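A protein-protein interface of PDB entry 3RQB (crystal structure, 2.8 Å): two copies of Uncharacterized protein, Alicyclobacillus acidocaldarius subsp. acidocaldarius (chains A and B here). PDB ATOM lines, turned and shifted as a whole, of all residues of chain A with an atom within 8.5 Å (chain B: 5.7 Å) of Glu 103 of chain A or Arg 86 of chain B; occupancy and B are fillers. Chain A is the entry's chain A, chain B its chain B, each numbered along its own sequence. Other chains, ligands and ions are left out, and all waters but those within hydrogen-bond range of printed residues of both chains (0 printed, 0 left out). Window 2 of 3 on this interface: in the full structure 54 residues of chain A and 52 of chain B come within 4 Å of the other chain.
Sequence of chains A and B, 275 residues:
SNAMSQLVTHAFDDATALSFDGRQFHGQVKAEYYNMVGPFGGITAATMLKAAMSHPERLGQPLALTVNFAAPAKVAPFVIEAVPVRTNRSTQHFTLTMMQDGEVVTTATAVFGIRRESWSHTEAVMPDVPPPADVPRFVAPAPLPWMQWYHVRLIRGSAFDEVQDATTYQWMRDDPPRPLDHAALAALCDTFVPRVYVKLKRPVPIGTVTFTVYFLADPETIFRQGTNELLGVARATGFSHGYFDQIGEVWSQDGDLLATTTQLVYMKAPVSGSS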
ATOM      1  N   ASN A  68     -22.111  17.638   7.366  1.00  0.00           N
ATOM      2  CA  ASN A  68     -23.483  17.873   7.784  1.00  0.00           C
ATOM      3  C   ASN A  68     -24.403  16.945   7.016  1.00  0.00           C
ATOM      4  O   ASN A  68     -24.289  16.812   5.799  1.00  0.00           O
ATOM      5  CB  ASN A  68     -23.869  19.331   7.530  1.00  0.00           C
ATOM      6  CG  ASN A  68     -22.724  20.287   7.815  1.00  0.00           C
ATOM      7  OD1 ASN A  68     -21.885  20.543   6.948  1.00  0.00           O
ATOM      8  ND2 ASN A  68     -22.672  20.806   9.038  1.00  0.00           N
ATOM      9  N   PHE A  69     -25.318  16.291   7.711  1.00  0.00           N
ATOM     10  CA  PHE A  69     -26.234  15.432   6.998  1.00  0.00           C
ATOM     11  C   PHE A  69     -27.543  16.172   6.851  1.00  0.00           C
ATOM     12  O   PHE A  69     -28.329  16.252   7.788  1.00  0.00           O
ATOM     13  CB  PHE A  69     -26.422  14.151   7.790  1.00  0.00           C
ATOM     14  CG  PHE A  69     -25.136  13.579   8.285  1.00  0.00           C
ATOM     15  CD1 PHE A  69     -24.459  12.621   7.545  1.00  0.00           C
ATOM     16  CD2 PHE A  69     -24.577  14.030   9.468  1.00  0.00           C
ATOM     17  CE1 PHE A  69     -23.259  12.103   7.986  1.00  0.00           C
ATOM     18  CE2 PHE A  69     -23.380  13.519   9.918  1.00  0.00           C
ATOM     19  CZ  PHE A  69     -22.715  12.555   9.174  1.00  0.00           C
ATOM     20  N   ALA A  70     -27.788  16.669   5.644  1.00  0.00           N
ATOM     21  CA  ALA A  70     -28.954  17.481   5.382  1.00  0.00           C
ATOM     22  C   ALA A  70     -30.169  16.579   5.480  1.00  0.00           C
ATOM     23  O   ALA A  70     -31.176  16.905   6.123  1.00  0.00           O
ATOM     24  CB  ALA A  70     -28.854  18.081   4.009  1.00  0.00           C
ATOM     25  N   ALA A  71     -30.052  15.429   4.836  1.00  0.00           N
ATOM     26  CA  ALA A  71     -31.095  14.433   4.863  1.00  0.00           C
ATOM     27  C   ALA A  71     -30.411  13.083   4.863  1.00  0.00           C
ATOM     28  O   ALA A  71     -29.331  12.940   4.281  1.00  0.00           O
ATOM     29  CB  ALA A  71     -31.971  14.584   3.642  1.00  0.00           C
ATOM     30  N   PRO A  72     -31.020  12.090   5.527  1.00  0.00           N
ATOM     31  CA  PRO A  72     -30.494  10.719   5.451  1.00  0.00           C
ATOM     32  C   PRO A  72     -30.533  10.239   4.000  1.00  0.00           C
ATOM     33  O   PRO A  72     -31.585  10.349   3.355  1.00  0.00           O
ATOM     34  CB  PRO A  72     -31.484   9.919   6.297  1.00  0.00           C
ATOM     35  CG  PRO A  72     -32.756  10.760   6.291  1.00  0.00           C
ATOM     36  CD  PRO A  72     -32.270  12.172   6.302  1.00  0.00           C
ATOM     37  N   ALA A  73     -29.410   9.729   3.494  1.00  0.00           N
ATOM     38  CA  ALA A  73     -29.333   9.314   2.093  1.00  0.00           C
ATOM     39  C   ALA A  73     -30.067   8.008   1.851  1.00  0.00           C
ATOM     40  O   ALA A  73     -30.007   7.099   2.676  1.00  0.00           O
ATOM     41  CB  ALA A  73     -27.910   9.175   1.671  1.00  0.00           C
ATOM     42  N   PHE A  78     -25.353   8.214  -6.153  1.00  0.00           N
ATOM     43  CA  PHE A  78     -25.264   9.634  -5.853  1.00  0.00           C
ATOM     44  C   PHE A  78     -24.124  10.255  -6.633  1.00  0.00           C
ATOM     45  O   PHE A  78     -23.274   9.542  -7.181  1.00  0.00           O
ATOM     46  CB  PHE A  78     -25.002   9.842  -4.373  1.00  0.00           C
ATOM     47  CG  PHE A  78     -23.736   9.218  -3.898  1.00  0.00           C
ATOM     48  CD1 PHE A  78     -22.518   9.850  -4.104  1.00  0.00           C
ATOM     49  CD2 PHE A  78     -23.757   8.002  -3.239  1.00  0.00           C
ATOM     50  CE1 PHE A  78     -21.344   9.281  -3.664  1.00  0.00           C
ATOM     51  CE2 PHE A  78     -22.590   7.429  -2.800  1.00  0.00           C
ATOM     52  CZ  PHE A  78     -21.376   8.073  -3.012  1.00  0.00           C
ATOM     53  N   VAL A  79     -24.113  11.585  -6.683  1.00  0.00           N
ATOM     54  CA  VAL A  79     -22.962  12.308  -7.196  1.00  0.00           C
ATOM     55  C   VAL A  79     -22.404  13.180  -6.087  1.00  0.00           C
ATOM     56  O   VAL A  79     -23.136  13.580  -5.176  1.00  0.00           O
ATOM     57  CB  VAL A  79     -23.322  13.190  -8.392  1.00  0.00           C
ATOM     58  CG1 VAL A  79     -24.333  12.480  -9.266  1.00  0.00           C
ATOM     59  CG2 VAL A  79     -23.867  14.529  -7.913  1.00  0.00           C
ATOM     60  N   THR A  97     -20.336  18.404  -1.793  1.00  0.00           N
ATOM     61  CA  THR A  97     -21.777  18.244  -1.751  1.00  0.00           C
ATOM     62  C   THR A  97     -22.212  16.926  -2.357  1.00  0.00           C
ATOM     63  O   THR A  97     -22.008  16.676  -3.546  1.00  0.00           O
ATOM     64  CB  THR A  97     -22.499  19.402  -2.486  1.00  0.00           C
ATOM     65  OG1 THR A  97     -22.504  20.575  -1.659  1.00  0.00           O
ATOM     66  CG2 THR A  97     -23.926  19.025  -2.774  1.00  0.00           C
ATOM     67  N   MET A  98     -22.831  16.089  -1.541  1.00  0.00           N
ATOM     68  CA  MET A  98     -23.415  14.871  -2.048  1.00  0.00           C
ATOM     69  C   MET A  98     -24.849  15.141  -2.467  1.00  0.00           C
ATOM     70  O   MET A  98     -25.587  15.842  -1.767  1.00  0.00           O
ATOM     71  CB  MET A  98     -23.388  13.785  -0.982  1.00  0.00           C
ATOM     72  CG  MET A  98     -24.133  12.534  -1.391  1.00  0.00           C
ATOM     73  SD  MET A  98     -23.900  11.135  -0.074  1.00  0.00           S
ATOM     74  CE  MET A  98     -21.960  11.088  -0.027  1.00  0.00           C
ATOM     75  N   MET A  99     -25.247  14.593  -3.610  1.00  0.00           N
ATOM     76  CA  MET A  99     -26.615  14.768  -4.086  1.00  0.00           C
ATOM     77  C   MET A  99     -27.219  13.481  -4.597  1.00  0.00           C
ATOM     78  O   MET A  99     -26.587  12.740  -5.349  1.00  0.00           O
ATOM     79  CB  MET A  99     -26.693  15.826  -5.175  1.00  0.00           C
ATOM     80  CG  MET A  99     -26.848  17.239  -4.646  1.00  0.00           C
ATOM     81  SD  MET A  99     -26.714  18.551  -6.091  1.00  0.00           S
ATOM     82  CE  MET A  99     -24.980  17.948  -6.753  1.00  0.00           C
ATOM     83  N   GLN A 100     -28.452  13.226  -4.172  1.00  0.00           N
ATOM     84  CA  GLN A 100     -29.249  12.145  -4.719  1.00  0.00           C
ATOM     85  C   GLN A 100     -30.512  12.722  -5.353  1.00  0.00           C
ATOM     86  O   GLN A 100     -31.390  13.235  -4.657  1.00  0.00           O
ATOM     87  CB  GLN A 100     -29.584  11.118  -3.638  1.00  0.00           C
ATOM     88  CG  GLN A 100     -28.507  10.071  -3.477  1.00  0.00           C
ATOM     89  CD  GLN A 100     -28.784   9.084  -2.361  1.00  0.00           C
ATOM     90  OE1 GLN A 100     -28.488   7.890  -2.481  1.00  0.00           O
ATOM     91  NE2 GLN A 100     -29.340   9.578  -1.260  1.00  0.00           N
ATOM     92  N   ASP A 101     -30.583  12.635  -6.678  1.00  0.00           N
ATOM     93  CA  ASP A 101     -31.709  13.156  -7.450  1.00  0.00           C
ATOM     94  C   ASP A 101     -31.822  14.677  -7.404  1.00  0.00           C
ATOM     95  O   ASP A 101     -32.921  15.231  -7.349  1.00  0.00           O
ATOM     96  CB  ASP A 101     -33.030  12.509  -7.009  1.00  0.00           C
ATOM     97  CG  ASP A 101     -33.185  11.078  -7.521  1.00  0.00           C
ATOM     98  OD1 ASP A 101     -32.642  10.757  -8.604  1.00  0.00           O
ATOM     99  OD2 ASP A 101     -33.856  10.276  -6.836  1.00  0.00           O
ATOM    100  N   GLY A 102     -30.680  15.351  -7.430  1.00  0.00           N
ATOM    101  CA  GLY A 102     -30.687  16.797  -7.498  1.00  0.00           C
ATOM    102  C   GLY A 102     -31.101  17.487  -6.211  1.00  0.00           C
ATOM    103  O   GLY A 102     -31.063  18.715  -6.130  1.00  0.00           O
ATOM    104  N   GLU A 103     -31.518  16.711  -5.214  1.00  0.00           N
ATOM    105  CA  GLU A 103     -31.721  17.237  -3.866  1.00  0.00           C
ATOM    106  C   GLU A 103     -30.479  16.940  -3.015  1.00  0.00           C
ATOM    107  O   GLU A 103     -29.944  15.826  -3.051  1.00  0.00           O
ATOM    108  CB  GLU A 103     -32.978  16.634  -3.216  1.00  0.00           C
ATOM    109  CG  GLU A 103     -34.312  17.113  -3.805  1.00  0.00           C
ATOM    110  CD  GLU A 103     -35.528  16.443  -3.158  1.00  0.00           C
ATOM    111  OE1 GLU A 103     -36.220  15.658  -3.849  1.00  0.00           O
ATOM    112  OE2 GLU A 103     -35.795  16.711  -1.964  1.00  0.00           O
ATOM    113  N   VAL A 104     -30.012  17.928  -2.254  1.00  0.00           N
ATOM    114  CA  VAL A 104     -28.826  17.715  -1.426  1.00  0.00           C
ATOM    115  C   VAL A 104     -29.063  16.837  -0.201  1.00  0.00           C
ATOM    116  O   VAL A 104     -29.948  17.084   0.622  1.00  0.00           O
ATOM    117  CB  VAL A 104     -28.168  19.016  -0.969  1.00  0.00           C
ATOM    118  CG1 VAL A 104     -27.041  18.700   0.025  1.00  0.00           C
ATOM    119  CG2 VAL A 104     -27.636  19.758  -2.161  1.00  0.00           C
ATOM    120  N   VAL A 105     -28.230  15.816  -0.098  1.00  0.00           N
ATOM    121  CA  VAL A 105     -28.264  14.864   0.988  1.00  0.00           C
ATOM    122  C   VAL A 105     -27.277  15.281   2.063  1.00  0.00           C
ATOM    123  O   VAL A 105     -27.615  15.359   3.251  1.00  0.00           O
ATOM    124  CB  VAL A 105     -27.928  13.466   0.503  1.00  0.00           C
ATOM    125  CG1 VAL A 105     -27.840  12.535   1.679  1.00  0.00           C
ATOM    126  CG2 VAL A 105     -28.989  12.988  -0.473  1.00  0.00           C
ATOM    127  N   THR A 106     -26.026  15.444   1.634  1.00  0.00           N
ATOM    128  CA  THR A 106     -24.916  15.711   2.534  1.00  0.00           C
ATOM    129  C   THR A 106     -23.943  16.770   2.017  1.00  0.00           C
ATOM    130  O   THR A 106     -23.653  16.829   0.825  1.00  0.00           O
ATOM    131  CB  THR A 106     -24.148  14.414   2.753  1.00  0.00           C
ATOM    132  OG1 THR A 106     -25.052  13.439   3.293  1.00  0.00           O
ATOM    133  CG2 THR A 106     -22.966  14.627   3.703  1.00  0.00           C
ATOM    134  N   THR A 107     -23.440  17.607   2.923  1.00  0.00           N
ATOM    135  CA  THR A 107     -22.348  18.537   2.601  1.00  0.00           C
ATOM    136  C   THR A 107     -21.150  18.335   3.523  1.00  0.00           C
ATOM    137  O   THR A 107     -21.245  17.680   4.569  1.00  0.00           O
ATOM    138  CB  THR A 107     -22.765  20.030   2.668  1.00  0.00           C
ATOM    139  OG1 THR A 107     -22.995  20.421   4.027  1.00  0.00           O
ATOM    140  CG2 THR A 107     -24.015  20.282   1.851  1.00  0.00           C
ATOM    141  N   PRO B  84     -29.179  28.309   1.314  1.00  0.00           N
ATOM    142  CA  PRO B  84     -30.076  27.436   2.069  1.00  0.00           C
ATOM    143  C   PRO B  84     -30.183  26.133   1.293  1.00  0.00           C
ATOM    144  O   PRO B  84     -31.090  25.895   0.501  1.00  0.00           O
ATOM    145  CB  PRO B  84     -31.396  28.203   2.065  1.00  0.00           C
ATOM    146  CG  PRO B  84     -31.369  28.921   0.776  1.00  0.00           C
ATOM    147  CD  PRO B  84     -29.921  29.320   0.550  1.00  0.00           C
ATOM    148  N   VAL B  85     -29.180  25.308   1.523  1.00  0.00           N
ATOM    149  CA  VAL B  85     -28.958  24.055   0.824  1.00  0.00           C
ATOM    150  C   VAL B  85     -30.038  22.951   1.023  1.00  0.00           C
ATOM    151  O   VAL B  85     -30.386  22.214   0.094  1.00  0.00           O
ATOM    152  CB  VAL B  85     -27.544  23.569   1.218  1.00  0.00           C
ATOM    153  CG1 VAL B  85     -27.468  22.046   1.385  1.00  0.00           C
ATOM    154  CG2 VAL B  85     -26.524  24.136   0.237  1.00  0.00           C
ATOM    155  N   ARG B  86     -30.568  22.825   2.228  1.00  0.00           N
ATOM    156  CA  ARG B  86     -31.605  21.841   2.453  1.00  0.00           C
ATOM    157  C   ARG B  86     -32.569  22.395   3.468  1.00  0.00           C
ATOM    158  O   ARG B  86     -32.170  23.050   4.423  1.00  0.00           O
ATOM    159  CB  ARG B  86     -31.007  20.531   2.965  1.00  0.00           C
ATOM    160  CG  ARG B  86     -31.994  19.392   2.967  1.00  0.00           C
ATOM    161  CD  ARG B  86     -32.673  19.324   1.611  1.00  0.00           C
ATOM    162  NE  ARG B  86     -33.786  18.387   1.609  1.00  0.00           N
ATOM    163  CZ  ARG B  86     -33.666  17.083   1.380  1.00  0.00           C
ATOM    164  NH1 ARG B  86     -32.477  16.558   1.127  1.00  0.00           N
ATOM    165  NH2 ARG B  86     -34.740  16.308   1.402  1.00  0.00           N
ATOM    166  N   THR B  87     -33.848  22.138   3.263  1.00  0.00           N
ATOM    167  CA  THR B  87     -34.839  22.610   4.209  1.00  0.00           C
ATOM    168  C   THR B  87     -35.825  21.494   4.552  1.00  0.00           C
ATOM    169  O   THR B  87     -36.421  20.850   3.675  1.00  0.00           O
ATOM    170  CB  THR B  87     -35.552  23.873   3.696  1.00  0.00           C
ATOM    171  OG1 THR B  87     -34.587  24.767   3.127  1.00  0.00           O
ATOM    172  CG2 THR B  87     -36.239  24.576   4.840  1.00  0.00           C
ATOM    173  N   ASN B  88     -35.967  21.257   5.848  1.00  0.00           N
ATOM    174  CA  ASN B  88     -36.782  20.160   6.333  1.00  0.00           C
ATOM    175  C   ASN B  88     -37.775  20.692   7.357  1.00  0.00           C
ATOM    176  O   ASN B  88     -37.795  21.896   7.619  1.00  0.00           O
ATOM    177  CB  ASN B  88     -35.875  19.076   6.907  1.00  0.00           C
ATOM    178  CG  ASN B  88     -34.734  18.713   5.956  1.00  0.00           C
ATOM    179  OD1 ASN B  88     -34.915  18.670   4.737  1.00  0.00           O
ATOM    180  ND2 ASN B  88     -33.555  18.466   6.510  1.00  0.00           N
ATOM    181  N   THR B  91     -35.693  21.536  10.532  1.00  0.00           N
ATOM    182  CA  THR B  91     -34.242  21.704  10.395  1.00  0.00           C
ATOM    183  C   THR B  91     -33.747  22.238   9.029  1.00  0.00           C
ATOM    184  O   THR B  91     -34.347  21.957   7.989  1.00  0.00           O
ATOM    185  CB  THR B  91     -33.557  20.373  10.749  1.00  0.00           C
ATOM    186  OG1 THR B  91     -32.292  20.626  11.357  1.00  0.00           O
ATOM    187  CG2 THR B  91     -33.392  19.487   9.518  1.00  0.00           C
ATOM    188  N   GLN B  92     -32.658  23.012   9.042  1.00  0.00           N
ATOM    189  CA  GLN B  92     -32.147  23.693   7.836  1.00  0.00           C
ATOM    190  C   GLN B  92     -30.603  23.796   7.745  1.00  0.00           C
ATOM    191  O   GLN B  92     -29.946  24.174   8.718  1.00  0.00           O
ATOM    192  CB  GLN B  92     -32.748  25.094   7.764  1.00  0.00           C
ATOM    193  CG  GLN B  92     -32.626  25.758   6.411  1.00  0.00           C
ATOM    194  CD  GLN B  92     -33.101  27.193   6.440  1.00  0.00           C
ATOM    195  OE1 GLN B  92     -33.144  27.820   7.498  1.00  0.00           O
ATOM    196  NE2 GLN B  92     -33.461  27.723   5.279  1.00  0.00           N
ATOM    197  N   HIS B  93     -30.035  23.506   6.571  1.00  0.00           N
ATOM    198  CA  HIS B  93     -28.576  23.525   6.387  1.00  0.00           C
ATOM    199  C   HIS B  93     -28.102  24.606   5.410  1.00  0.00           C
ATOM    200  O   HIS B  93     -28.627  24.711   4.299  1.00  0.00           O
ATOM    201  CB  HIS B  93     -28.080  22.181   5.851  1.00  0.00           C
ATOM    202  CG  HIS B  93     -28.057  21.083   6.864  1.00  0.00           C
ATOM    203  ND1 HIS B  93     -29.199  20.440   7.294  1.00  0.00           N
ATOM    204  CD2 HIS B  93     -27.023  20.488   7.508  1.00  0.00           C
ATOM    205  CE1 HIS B  93     -28.872  19.505   8.168  1.00  0.00           C
ATOM    206  NE2 HIS B  93     -27.559  19.513   8.317  1.00  0.00           N
ATOM    207  N   PHE B  94     -27.082  25.371   5.803  1.00  0.00           N
ATOM    208  CA  PHE B  94     -26.531  26.436   4.954  1.00  0.00           C
ATOM    209  C   PHE B  94     -25.096  26.180   4.525  1.00  0.00           C
ATOM    210  O   PHE B  94     -24.310  25.594   5.268  1.00  0.00           O
ATOM    211  CB  PHE B  94     -26.571  27.785   5.676  1.00  0.00           C
ATOM    212  CG  PHE B  94     -27.919  28.442   5.663  1.00  0.00           C
ATOM    213  CD1 PHE B  94     -28.879  28.104   6.605  1.00  0.00           C
ATOM    214  CD2 PHE B  94     -28.225  29.409   4.715  1.00  0.00           C
ATOM    215  CE1 PHE B  94     -30.126  28.708   6.592  1.00  0.00           C
ATOM    216  CE2 PHE B  94     -29.470  30.020   4.699  1.00  0.00           C
ATOM    217  CZ  PHE B  94     -30.424  29.665   5.639  1.00  0.00           C
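No position is printed for both chains.
Of the 10 pairs that touch across the chains among the printed residues, none has its exchanged pair printed and touching as well.
Among the printed residues, merely in contact across the chains: Ala 71 of chain A with Arg 86 of chain B (3.2 Å), Asn 68 of chain A with His 93 of chain B (3.4 Å), Ala 70 of chain A with Arg 86 of chain B (3.4 Å), Ala 70 of chain A with His 93 of chain B (3.4 Å), Val 104 of chain A with Val 85 of chain B (3.6 Å) and Thr 107 of chain A with Val 85 of chain B (3.9 Å).
The backbone carbonyl oxygen (O) of Thr 107 of chain A is in hydrogen-bond range of the backbone NH (N) of Asn 68 of chain A, at 2.9 Å.
The backbone carbonyl oxygen (O) of Arg 86 of chain B is in hydrogen-bond range of the backbone NH (N) of His 93 of chain B (3.1 Å).
The backbone NH of Val 85 of chain B is in hydrogen-bond range of the backbone carbonyl oxygen of His 93 of chain B (2.9 Å).
The guanidinium group (NE) of Arg 86 of chain B sits at hydrogen-bond distance from the side-chain amide oxygen (OD1) of Asn 88 of chain B (3.3 Å).
O of Val 105 of chain A lies within hydrogen-bond range of N of Ala 71 of chain A.
The backbone NH (N) of Ala 70 of chain A lies within hydrogen-bond range of the backbone carbonyl oxygen (O) of Val 105 of chain A, at 2.7 Å.
Of the 19 printed residues of chain A, 7 touch a printed residue of chain B.
Among the printed residues, 10 pairs touch across the chains.
O of Phe 69 of chain A sits close to NE2 of His 93 of chain B.
The backbone carbonyl oxygen (O) of Ala 70 of chain A is in hydrogen-bond range of the side-chain amide nitrogen (ND2) of Asn 88 of chain B (2.9 Å).
OE2 of Glu 103 of chain A lies within salt-bridge range of NH2 of Arg 86 of chain B (3.6 Å).
The backbone carbonyl oxygen of Val 104 of chain A lies within hydrogen-bond range of the guanidinium group of Arg 86 of chain B, at 2.6 Å.
Glu 103 of chain A touches one residue of chain B.
Arg 86 of chain B touches four residues of chain A.
No residue of chain A comes within 4 Å of Thr 87 of chain B.
Of the printed residues of chain B, Val 104 of chain A touches Val 85 (3.6 Å) and Arg 86 (2.6 Å).
Of the printed residues of chain B, Phe 69 of chain A touches His 93 (3.3 Å).
Printed residues of chain B within 4 Å of Ala 70 of chain A: Arg 86, Asn 88 and His 93.
Of the printed residues of chain A, Asn 88 of chain B touches Ala 70 (2.9 Å).
Of the printed residues of chain B, Thr 107 of chain A touches Val 85.
Gln 92 of chain B touches none of the printed residues of chain A.
The nearest printed residue of chain B that does not touch Glu 103 of chain A is Val 85 of chain B (6.1 Å).
The nearest residue of chain A that does not touch Arg 86 of chain B is Val 105 of chain A (4.5 Å).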
